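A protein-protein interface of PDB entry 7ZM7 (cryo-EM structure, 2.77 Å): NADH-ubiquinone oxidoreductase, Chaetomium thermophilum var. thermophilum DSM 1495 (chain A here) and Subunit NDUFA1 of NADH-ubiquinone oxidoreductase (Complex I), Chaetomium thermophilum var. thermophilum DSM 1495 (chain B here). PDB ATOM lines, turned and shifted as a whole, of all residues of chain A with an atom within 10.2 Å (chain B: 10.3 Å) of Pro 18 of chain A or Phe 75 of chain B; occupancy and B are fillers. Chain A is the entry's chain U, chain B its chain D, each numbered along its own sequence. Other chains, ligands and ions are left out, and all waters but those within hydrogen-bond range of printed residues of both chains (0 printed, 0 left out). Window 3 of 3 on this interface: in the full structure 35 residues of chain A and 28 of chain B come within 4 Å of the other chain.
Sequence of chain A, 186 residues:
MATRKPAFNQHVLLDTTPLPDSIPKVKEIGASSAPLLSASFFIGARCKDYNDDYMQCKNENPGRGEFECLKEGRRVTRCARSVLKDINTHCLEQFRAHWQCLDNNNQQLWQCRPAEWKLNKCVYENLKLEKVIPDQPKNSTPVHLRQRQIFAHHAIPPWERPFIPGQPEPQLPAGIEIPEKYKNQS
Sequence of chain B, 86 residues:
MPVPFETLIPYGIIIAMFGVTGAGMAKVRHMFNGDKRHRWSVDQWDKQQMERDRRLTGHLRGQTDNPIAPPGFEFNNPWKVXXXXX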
ATOM      1  N   VAL A  12      37.070  10.790 -28.010  1.00  0.00           N
ATOM      2  CA  VAL A  12      36.117  10.988 -26.924  1.00  0.00           C
ATOM      3  C   VAL A  12      36.728  10.445 -25.644  1.00  0.00           C
ATOM      4  O   VAL A  12      37.358   9.385 -25.659  1.00  0.00           O
ATOM      5  CB  VAL A  12      34.769  10.310 -27.221  1.00  0.00           C
ATOM      6  CG1 VAL A  12      33.966  10.173 -25.963  1.00  0.00           C
ATOM      7  CG2 VAL A  12      33.993  11.127 -28.236  1.00  0.00           C
ATOM      8  N   LEU A  13      36.564  11.174 -24.546  1.00  0.00           N
ATOM      9  CA  LEU A  13      37.074  10.756 -23.246  1.00  0.00           C
ATOM     10  C   LEU A  13      35.917  10.429 -22.309  1.00  0.00           C
ATOM     11  O   LEU A  13      35.202  11.326 -21.863  1.00  0.00           O
ATOM     12  CB  LEU A  13      37.970  11.827 -22.643  1.00  0.00           C
ATOM     13  CG  LEU A  13      38.413  11.587 -21.210  1.00  0.00           C
ATOM     14  CD1 LEU A  13      39.349  10.411 -21.103  1.00  0.00           C
ATOM     15  CD2 LEU A  13      39.071  12.815 -20.699  1.00  0.00           C
ATOM     16  N   LEU A  14      35.769   9.148 -21.969  1.00  0.00           N
ATOM     17  CA  LEU A  14      34.673   8.656 -21.097  1.00  0.00           C
ATOM     18  C   LEU A  14      35.215   8.405 -19.691  1.00  0.00           C
ATOM     19  O   LEU A  14      36.367   8.002 -19.578  1.00  0.00           O
ATOM     20  CB  LEU A  14      34.076   7.378 -21.693  1.00  0.00           C
ATOM     21  CG  LEU A  14      33.147   7.552 -22.890  1.00  0.00           C
ATOM     22  CD1 LEU A  14      32.299   6.308 -23.083  1.00  0.00           C
ATOM     23  CD2 LEU A  14      32.251   8.762 -22.708  1.00  0.00           C
ATOM     24  N   ASP A  15      34.461   8.751 -18.655  1.00  0.00           N
ATOM     25  CA  ASP A  15      34.905   8.406 -17.277  1.00  0.00           C
ATOM     26  C   ASP A  15      33.909   7.396 -16.700  1.00  0.00           C
ATOM     27  O   ASP A  15      32.739   7.746 -16.578  1.00  0.00           O
ATOM     28  CB  ASP A  15      35.094   9.661 -16.417  1.00  0.00           C
ATOM     29  CG  ASP A  15      36.102   9.477 -15.305  1.00  0.00           C
ATOM     30  OD1 ASP A  15      36.714   8.402 -15.254  1.00  0.00           O
ATOM     31  OD2 ASP A  15      36.262  10.413 -14.500  1.00  0.00           O
ATOM     32  N   THR A  16      34.357   6.177 -16.396  1.00  0.00           N
ATOM     33  CA  THR A  16      33.419   5.120 -15.928  1.00  0.00           C
ATOM     34  C   THR A  16      33.214   5.232 -14.415  1.00  0.00           C
ATOM     35  O   THR A  16      32.439   4.432 -13.867  1.00  0.00           O
ATOM     36  CB  THR A  16      33.900   3.724 -16.337  1.00  0.00           C
ATOM     37  OG1 THR A  16      35.082   3.434 -15.588  1.00  0.00           O
ATOM     38  CG2 THR A  16      34.176   3.608 -17.819  1.00  0.00           C
ATOM     39  N   THR A  17      33.872   6.203 -13.779  1.00  0.00           N
ATOM     40  CA  THR A  17      33.759   6.377 -12.311  1.00  0.00           C
ATOM     41  C   THR A  17      32.312   6.733 -11.970  1.00  0.00           C
ATOM     42  O   THR A  17      31.764   7.624 -12.622  1.00  0.00           O
ATOM     43  CB  THR A  17      34.753   7.441 -11.835  1.00  0.00           C
ATOM     44  OG1 THR A  17      35.921   7.362 -12.650  1.00  0.00           O
ATOM     45  CG2 THR A  17      35.130   7.290 -10.377  1.00  0.00           C
ATOM     46  N   PRO A  18      31.667   6.085 -10.976  1.00  0.00           N
ATOM     47  CA  PRO A  18      30.263   6.343 -10.677  1.00  0.00           C
ATOM     48  C   PRO A  18      30.054   7.572  -9.787  1.00  0.00           C
ATOM     49  O   PRO A  18      30.999   8.005  -9.159  1.00  0.00           O
ATOM     50  CB  PRO A  18      29.815   5.090  -9.917  1.00  0.00           C
ATOM     51  CG  PRO A  18      30.988   4.133  -9.995  1.00  0.00           C
ATOM     52  CD  PRO A  18      32.210   5.010 -10.154  1.00  0.00           C
ATOM     53  N   LEU A  19      28.831   8.105  -9.752  1.00  0.00           N
ATOM     54  CA  LEU A  19      28.535   9.237  -8.845  1.00  0.00           C
ATOM     55  C   LEU A  19      28.654   8.699  -7.422  1.00  0.00           C
ATOM     56  O   LEU A  19      28.413   7.500  -7.224  1.00  0.00           O
ATOM     57  CB  LEU A  19      27.113   9.724  -9.128  1.00  0.00           C
ATOM     58  CG  LEU A  19      26.978  10.965 -10.007  1.00  0.00           C
ATOM     59  CD1 LEU A  19      25.680  10.937 -10.797  1.00  0.00           C
ATOM     60  CD2 LEU A  19      27.074  12.237  -9.183  1.00  0.00           C
ATOM     61  N   PRO A  20      29.017   9.512  -6.416  1.00  0.00           N
ATOM     62  CA  PRO A  20      29.236   9.003  -5.071  1.00  0.00           C
ATOM     63  C   PRO A  20      27.913   8.529  -4.446  1.00  0.00           C
ATOM     64  O   PRO A  20      26.870   8.933  -4.930  1.00  0.00           O
ATOM     65  CB  PRO A  20      29.850  10.198  -4.345  1.00  0.00           C
ATOM     66  CG  PRO A  20      30.328  11.101  -5.443  1.00  0.00           C
ATOM     67  CD  PRO A  20      29.284  10.939  -6.521  1.00  0.00           C
ATOM     68  N   ASP A  21      27.966   7.722  -3.381  1.00  0.00           N
ATOM     69  CA  ASP A  21      26.728   7.113  -2.819  1.00  0.00           C
ATOM     70  C   ASP A  21      26.029   8.159  -1.955  1.00  0.00           C
ATOM     71  O   ASP A  21      24.820   8.007  -1.699  1.00  0.00           O
ATOM     72  CB  ASP A  21      27.086   5.872  -2.001  1.00  0.00           C
ATOM     73  CG  ASP A  21      25.906   4.973  -1.677  1.00  0.00           C
ATOM     74  OD1 ASP A  21      24.900   5.045  -2.404  1.00  0.00           O
ATOM     75  OD2 ASP A  21      26.006   4.205  -0.701  1.00  0.00           O
ATOM     76  N   SER A  22      26.751   9.201  -1.559  1.00  0.00           N
ATOM     77  CA  SER A  22      26.162  10.301  -0.804  1.00  0.00           C
ATOM     78  C   SER A  22      24.994  10.937  -1.549  1.00  0.00           C
ATOM     79  O   SER A  22      23.986  11.298  -0.933  1.00  0.00           O
ATOM     80  CB  SER A  22      27.229  11.344  -0.488  1.00  0.00           C
ATOM     81  OG  SER A  22      28.266  10.779   0.292  1.00  0.00           O
ATOM     82  N   ILE A  23      25.112  11.097  -2.861  1.00  0.00           N
ATOM     83  CA  ILE A  23      24.075  11.746  -3.658  1.00  0.00           C
ATOM     84  C   ILE A  23      23.016  10.719  -4.045  1.00  0.00           C
ATOM     85  O   ILE A  23      23.337   9.725  -4.714  1.00  0.00           O
ATOM     86  CB  ILE A  23      24.676  12.412  -4.901  1.00  0.00           C
ATOM     87  CG1 ILE A  23      25.949  13.162  -4.527  1.00  0.00           C
ATOM     88  CG2 ILE A  23      23.668  13.346  -5.541  1.00  0.00           C
ATOM     89  CD1 ILE A  23      26.768  13.583  -5.698  1.00  0.00           C
ATOM     90  N   LYS A  25      20.598   8.491  -5.986  1.00  0.00           N
ATOM     91  CA  LYS A  25      20.602   8.184  -7.439  1.00  0.00           C
ATOM     92  C   LYS A  25      19.222   8.451  -8.043  1.00  0.00           C
ATOM     93  O   LYS A  25      18.231   8.422  -7.290  1.00  0.00           O
ATOM     94  CB  LYS A  25      20.999   6.724  -7.669  1.00  0.00           C
ATOM     95  CG  LYS A  25      20.136   5.695  -6.951  1.00  0.00           C
ATOM     96  CD  LYS A  25      20.558   4.268  -7.228  1.00  0.00           C
ATOM     97  CE  LYS A  25      21.987   3.984  -6.818  1.00  0.00           C
ATOM     98  NZ  LYS A  25      22.369   2.579  -7.099  1.00  0.00           N
ATOM     99  N   GLU A  28      17.474   7.747 -15.159  1.00  0.00           N
ATOM    100  CA  GLU A  28      17.530   8.878 -16.114  1.00  0.00           C
ATOM    101  C   GLU A  28      16.443   8.756 -17.179  1.00  0.00           C
ATOM    102  O   GLU A  28      15.896   7.652 -17.340  1.00  0.00           O
ATOM    103  CB  GLU A  28      18.917   8.929 -16.755  1.00  0.00           C
ATOM    104  CG  GLU A  28      20.043   9.136 -15.760  1.00  0.00           C
ATOM    105  CD  GLU A  28      20.198  10.561 -15.259  1.00  0.00           C
ATOM    106  OE1 GLU A  28      19.498  11.450 -15.781  1.00  0.00           O
ATOM    107  OE2 GLU A  28      21.023  10.779 -14.350  1.00  0.00           O
ATOM    108  N   ARG B  55      23.742   8.092 -27.850  1.00  0.00           N
ATOM    109  CA  ARG B  55      23.965   7.554 -26.520  1.00  0.00           C
ATOM    110  C   ARG B  55      22.925   6.509 -26.163  1.00  0.00           C
ATOM    111  O   ARG B  55      23.244   5.500 -25.532  1.00  0.00           O
ATOM    112  CB  ARG B  55      23.957   8.679 -25.494  1.00  0.00           C
ATOM    113  CG  ARG B  55      25.243   9.419 -25.404  1.00  0.00           C
ATOM    114  CD  ARG B  55      25.124  10.568 -24.463  1.00  0.00           C
ATOM    115  NE  ARG B  55      25.124  10.118 -23.087  1.00  0.00           N
ATOM    116  CZ  ARG B  55      24.361  10.627 -22.135  1.00  0.00           C
ATOM    117  NH1 ARG B  55      23.520  11.604 -22.414  1.00  0.00           N
ATOM    118  NH2 ARG B  55      24.434  10.153 -20.905  1.00  0.00           N
ATOM    119  N   LEU B  56      21.673   6.741 -26.533  1.00  0.00           N
ATOM    120  CA  LEU B  56      20.628   5.803 -26.153  1.00  0.00           C
ATOM    121  C   LEU B  56      20.563   4.608 -27.092  1.00  0.00           C
ATOM    122  O   LEU B  56      20.311   3.488 -26.646  1.00  0.00           O
ATOM    123  CB  LEU B  56      19.280   6.516 -26.093  1.00  0.00           C
ATOM    124  CG  LEU B  56      19.113   7.425 -24.886  1.00  0.00           C
ATOM    125  CD1 LEU B  56      18.014   8.426 -25.120  1.00  0.00           C
ATOM    126  CD2 LEU B  56      18.843   6.624 -23.650  1.00  0.00           C
ATOM    127  N   ALA B  69      16.129   5.241 -19.134  1.00  0.00           N
ATOM    128  CA  ALA B  69      17.346   5.011 -19.878  1.00  0.00           C
ATOM    129  C   ALA B  69      17.981   3.693 -19.436  1.00  0.00           C
ATOM    130  O   ALA B  69      17.880   3.306 -18.270  1.00  0.00           O
ATOM    131  CB  ALA B  69      18.314   6.163 -19.676  1.00  0.00           C
ATOM    132  N   PRO B  70      18.629   2.980 -20.351  1.00  0.00           N
ATOM    133  CA  PRO B  70      19.212   1.678 -20.014  1.00  0.00           C
ATOM    134  C   PRO B  70      20.465   1.827 -19.171  1.00  0.00           C
ATOM    135  O   PRO B  70      21.123   2.876 -19.200  1.00  0.00           O
ATOM    136  CB  PRO B  70      19.532   1.074 -21.386  1.00  0.00           C
ATOM    137  CG  PRO B  70      19.667   2.239 -22.278  1.00  0.00           C
ATOM    138  CD  PRO B  70      18.777   3.307 -21.774  1.00  0.00           C
ATOM    139  N   PRO B  71      20.826   0.796 -18.404  1.00  0.00           N
ATOM    140  CA  PRO B  71      21.997   0.902 -17.523  1.00  0.00           C
ATOM    141  C   PRO B  71      23.279   1.139 -18.303  1.00  0.00           C
ATOM    142  O   PRO B  71      23.518   0.533 -19.349  1.00  0.00           O
ATOM    143  CB  PRO B  71      22.019  -0.448 -16.800  1.00  0.00           C
ATOM    144  CG  PRO B  71      21.251  -1.359 -17.681  1.00  0.00           C
ATOM    145  CD  PRO B  71      20.182  -0.521 -18.302  1.00  0.00           C
ATOM    146  N   GLY B  72      24.125   2.002 -17.758  1.00  0.00           N
ATOM    147  CA  GLY B  72      25.280   2.495 -18.464  1.00  0.00           C
ATOM    148  C   GLY B  72      25.084   3.838 -19.129  1.00  0.00           C
ATOM    149  O   GLY B  72      26.073   4.514 -19.413  1.00  0.00           O
ATOM    150  N   PHE B  73      23.840   4.263 -19.367  1.00  0.00           N
ATOM    151  CA  PHE B  73      23.566   5.554 -20.058  1.00  0.00           C
ATOM    152  C   PHE B  73      24.276   6.701 -19.340  1.00  0.00           C
ATOM    153  O   PHE B  73      24.774   7.619 -19.999  1.00  0.00           O
ATOM    154  CB  PHE B  73      22.066   5.855 -20.083  1.00  0.00           C
ATOM    155  CG  PHE B  73      21.699   7.175 -20.708  1.00  0.00           C
ATOM    156  CD1 PHE B  73      21.941   7.413 -22.050  1.00  0.00           C
ATOM    157  CD2 PHE B  73      21.126   8.184 -19.954  1.00  0.00           C
ATOM    158  CE1 PHE B  73      21.614   8.629 -22.623  1.00  0.00           C
ATOM    159  CE2 PHE B  73      20.787   9.396 -20.532  1.00  0.00           C
ATOM    160  CZ  PHE B  73      21.031   9.616 -21.866  1.00  0.00           C
ATOM    161  N   GLU B  74      24.355   6.631 -18.012  1.00  0.00           N
ATOM    162  CA  GLU B  74      24.971   7.713 -17.209  1.00  0.00           C
ATOM    163  C   GLU B  74      26.447   7.946 -17.601  1.00  0.00           C
ATOM    164  O   GLU B  74      26.885   9.101 -17.496  1.00  0.00           O
ATOM    165  CB  GLU B  74      24.812   7.345 -15.742  1.00  0.00           C
ATOM    166  CG  GLU B  74      25.035   5.870 -15.458  1.00  0.00           C
ATOM    167  CD  GLU B  74      23.780   5.027 -15.308  1.00  0.00           C
ATOM    168  OE1 GLU B  74      23.107   4.774 -16.328  1.00  0.00           O
ATOM    169  OE2 GLU B  74      23.475   4.626 -14.169  1.00  0.00           O
ATOM    170  N   PHE B  75      27.199   6.912 -17.985  1.00  0.00           N
ATOM    171  CA  PHE B  75      28.651   7.049 -18.276  1.00  0.00           C
ATOM    172  C   PHE B  75      28.987   7.198 -19.769  1.00  0.00           C
ATOM    173  O   PHE B  75      30.173   7.397 -20.054  1.00  0.00           O
ATOM    174  CB  PHE B  75      29.372   5.784 -17.801  1.00  0.00           C
ATOM    175  CG  PHE B  75      29.011   5.345 -16.407  1.00  0.00           C
ATOM    176  CD1 PHE B  75      29.419   6.079 -15.308  1.00  0.00           C
ATOM    177  CD2 PHE B  75      28.262   4.199 -16.198  1.00  0.00           C
ATOM    178  CE1 PHE B  75      29.081   5.680 -14.027  1.00  0.00           C
ATOM    179  CE2 PHE B  75      27.926   3.802 -14.914  1.00  0.00           C
ATOM    180  CZ  PHE B  75      28.335   4.543 -13.832  1.00  0.00           C
ATOM    181  N   ASN B  76      28.018   7.122 -20.684  1.00  0.00           N
ATOM    182  CA  ASN B  76      28.319   7.138 -22.142  1.00  0.00           C
ATOM    183  C   ASN B  76      28.288   8.562 -22.691  1.00  0.00           C
ATOM    184  O   ASN B  76      28.463   8.711 -23.908  1.00  0.00           O
ATOM    185  CB  ASN B  76      27.466   6.150 -22.940  1.00  0.00           C
ATOM    186  CG  ASN B  76      25.973   6.382 -22.896  1.00  0.00           C
ATOM    187  OD1 ASN B  76      25.511   7.470 -22.580  1.00  0.00           O
ATOM    188  ND2 ASN B  76      25.207   5.364 -23.245  1.00  0.00           N
ATOM    189  N   ASN B  77      28.094   9.554 -21.823  1.00  0.00           N
ATOM    190  CA  ASN B  77      28.048  10.985 -22.224  1.00  0.00           C
ATOM    191  C   ASN B  77      29.400  11.316 -22.838  1.00  0.00           C
ATOM    192  O   ASN B  77      30.396  11.236 -22.110  1.00  0.00           O
ATOM    193  CB  ASN B  77      27.684  11.898 -21.053  1.00  0.00           C
ATOM    194  CG  ASN B  77      27.514  13.343 -21.469  1.00  0.00           C
ATOM    195  OD1 ASN B  77      27.031  13.624 -22.562  1.00  0.00           O
ATOM    196  ND2 ASN B  77      27.901  14.265 -20.606  1.00  0.00           N
ATOM    197  N   PRO B  78      29.486  11.729 -24.113  1.00  0.00           N
ATOM    198  CA  PRO B  78      30.780  11.915 -24.760  1.00  0.00           C
ATOM    199  C   PRO B  78      31.402  13.293 -24.525  1.00  0.00           C
ATOM    200  O   PRO B  78      30.778  14.277 -24.835  1.00  0.00           O
ATOM    201  CB  PRO B  78      30.437  11.706 -26.237  1.00  0.00           C
ATOM    202  CG  PRO B  78      28.975  12.100 -26.378  1.00  0.00           C
ATOM    203  CD  PRO B  78      28.362  12.036 -24.994  1.00  0.00           C
ATOM    204  N   TRP B  79      32.584  13.344 -23.914  1.00  0.00           N
ATOM    205  CA  TRP B  79      33.291  14.644 -23.797  1.00  0.00           C
ATOM    206  C   TRP B  79      34.371  14.641 -24.873  1.00  0.00           C
ATOM    207  O   TRP B  79      35.274  13.809 -24.792  1.00  0.00           O
ATOM    208  CB  TRP B  79      33.856  14.878 -22.390  1.00  0.00           C
ATOM    209  CG  TRP B  79      32.863  15.277 -21.343  1.00  0.00           C
ATOM    210  CD1 TRP B  79      31.508  15.135 -21.388  1.00  0.00           C
ATOM    211  CD2 TRP B  79      33.160  15.874 -20.069  1.00  0.00           C
ATOM    212  NE1 TRP B  79      30.943  15.610 -20.237  1.00  0.00           N
ATOM    213  CE2 TRP B  79      31.932  16.069 -19.409  1.00  0.00           C
ATOM    214  CE3 TRP B  79      34.340  16.257 -19.422  1.00  0.00           C
ATOM    215  CZ2 TRP B  79      31.850  16.637 -18.139  1.00  0.00           C
ATOM    216  CZ3 TRP B  79      34.260  16.815 -18.165  1.00  0.00           C
ATOM    217  CH2 TRP B  79      33.030  17.004 -17.536  1.00  0.00           C
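Of chain B, only Phe 75, Asn 76 and Asn 77 come within 4 Å of Leu 14 of chain A. Printed residues of chain B within 4 Å of Thr 17 of chain A: Phe 75. Pro 18 of chain A touches one residue of chain B. No residue of chain B comes within 4 Å of Pro 20 of chain A. Asp 21 of chain A touches none of the printed residues of chain B. Of the printed residues of chain A, Ala 69 of chain B touches Glu 28 (3.0 Å). Pro 70 of chain B touches none of the printed residues of chain A. No residue of chain A comes within 4 Å of Gly 72 of chain B. Of the printed residues of chain A, Phe 73 of chain B touches Glu 28 (3.96 Å). Glu 74 of chain B touches none of the printed residues of chain A. Of chain A, only Leu 14, Asp 15, Thr 16, Thr 17 and Pro 18 come within 4 Å of Phe 75 of chain B. Of chain A, only Leu 14 comes within 4 Å of Asn 76 of chain B. Of the printed residues of chain A, Trp 79 of chain B touches Val 12 and Leu 13. The nearest printed residue of chain A that does not touch Asn 77 of chain B is Leu 13 of chain A (4.8 Å).
Of the 14 printed residues of chain A, 8 touch a printed residue of chain B. Hydrophobic or aromatic side chains of chain A within 4 Å of the printed part of chain B: Val 12, Leu 13 and Leu 14. Along chain A the printed residues that touch a printed residue of chain B span positions 12 to 28. Of the 13 printed residues of chain B, 7 touch a printed residue of chain A. Hydrophobic or aromatic side chains of chain B within 4 Å of the printed part of chain A: Ala 69, Phe 73, Phe 75, Pro 78 and Trp 79. Among the printed residues, no Asp or Glu carboxylate lies within 4 Å of a Lys or Arg side-chain nitrogen of the other chain.
The backbone NH (N) of Leu 13 of chain A sits at hydrogen-bond distance from the backbone carbonyl oxygen (O) of Trp 79 of chain B (2.9 Å). O of Glu 28 of chain A lies within hydrogen-bond range of N of Ala 69 of chain B (3.0 Å).
Among the printed residues, pairs that only touch across the chains: Val 12 of chain A with Pro 78 of chain B, Val 12 of chain A with Trp 79 of chain B, Leu 14 of chain A with Phe 75 of chain B, Leu 14 of chain A with Asn 76 of chain B, Leu 14 of chain A with Asn 77 of chain B, Asp 15 of chain A with Phe 75 of chain B, Thr 16 of chain A with Phe 75 of chain B, Thr 17 of chain A with Phe 75 of chain B, Pro 18 of chain A with Phe 75 of chain B and Glu 28 of chain A with Phe 73 of chain B.
OD1 of Asp 15 of chain A is in hydrogen-bond range of OG1 of Thr 17 of chain A (2.9 Å). The backbone carbonyl oxygen (O) of Phe 73 of chain B sits close to the side-chain amide oxygen (OD1) of Asn 76 of chain B, 2.7 Å away. ND2 of Asn 77 of chain B sits close to NE1 of Trp 79 of chain B. NH2 of Arg 55 of chain B is in hydrogen-bond range of O of Phe 73 of chain B, at 2.7 Å. NE of Arg 55 of chain B lies within hydrogen-bond range of OD1 of Asn 76 of chain B.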
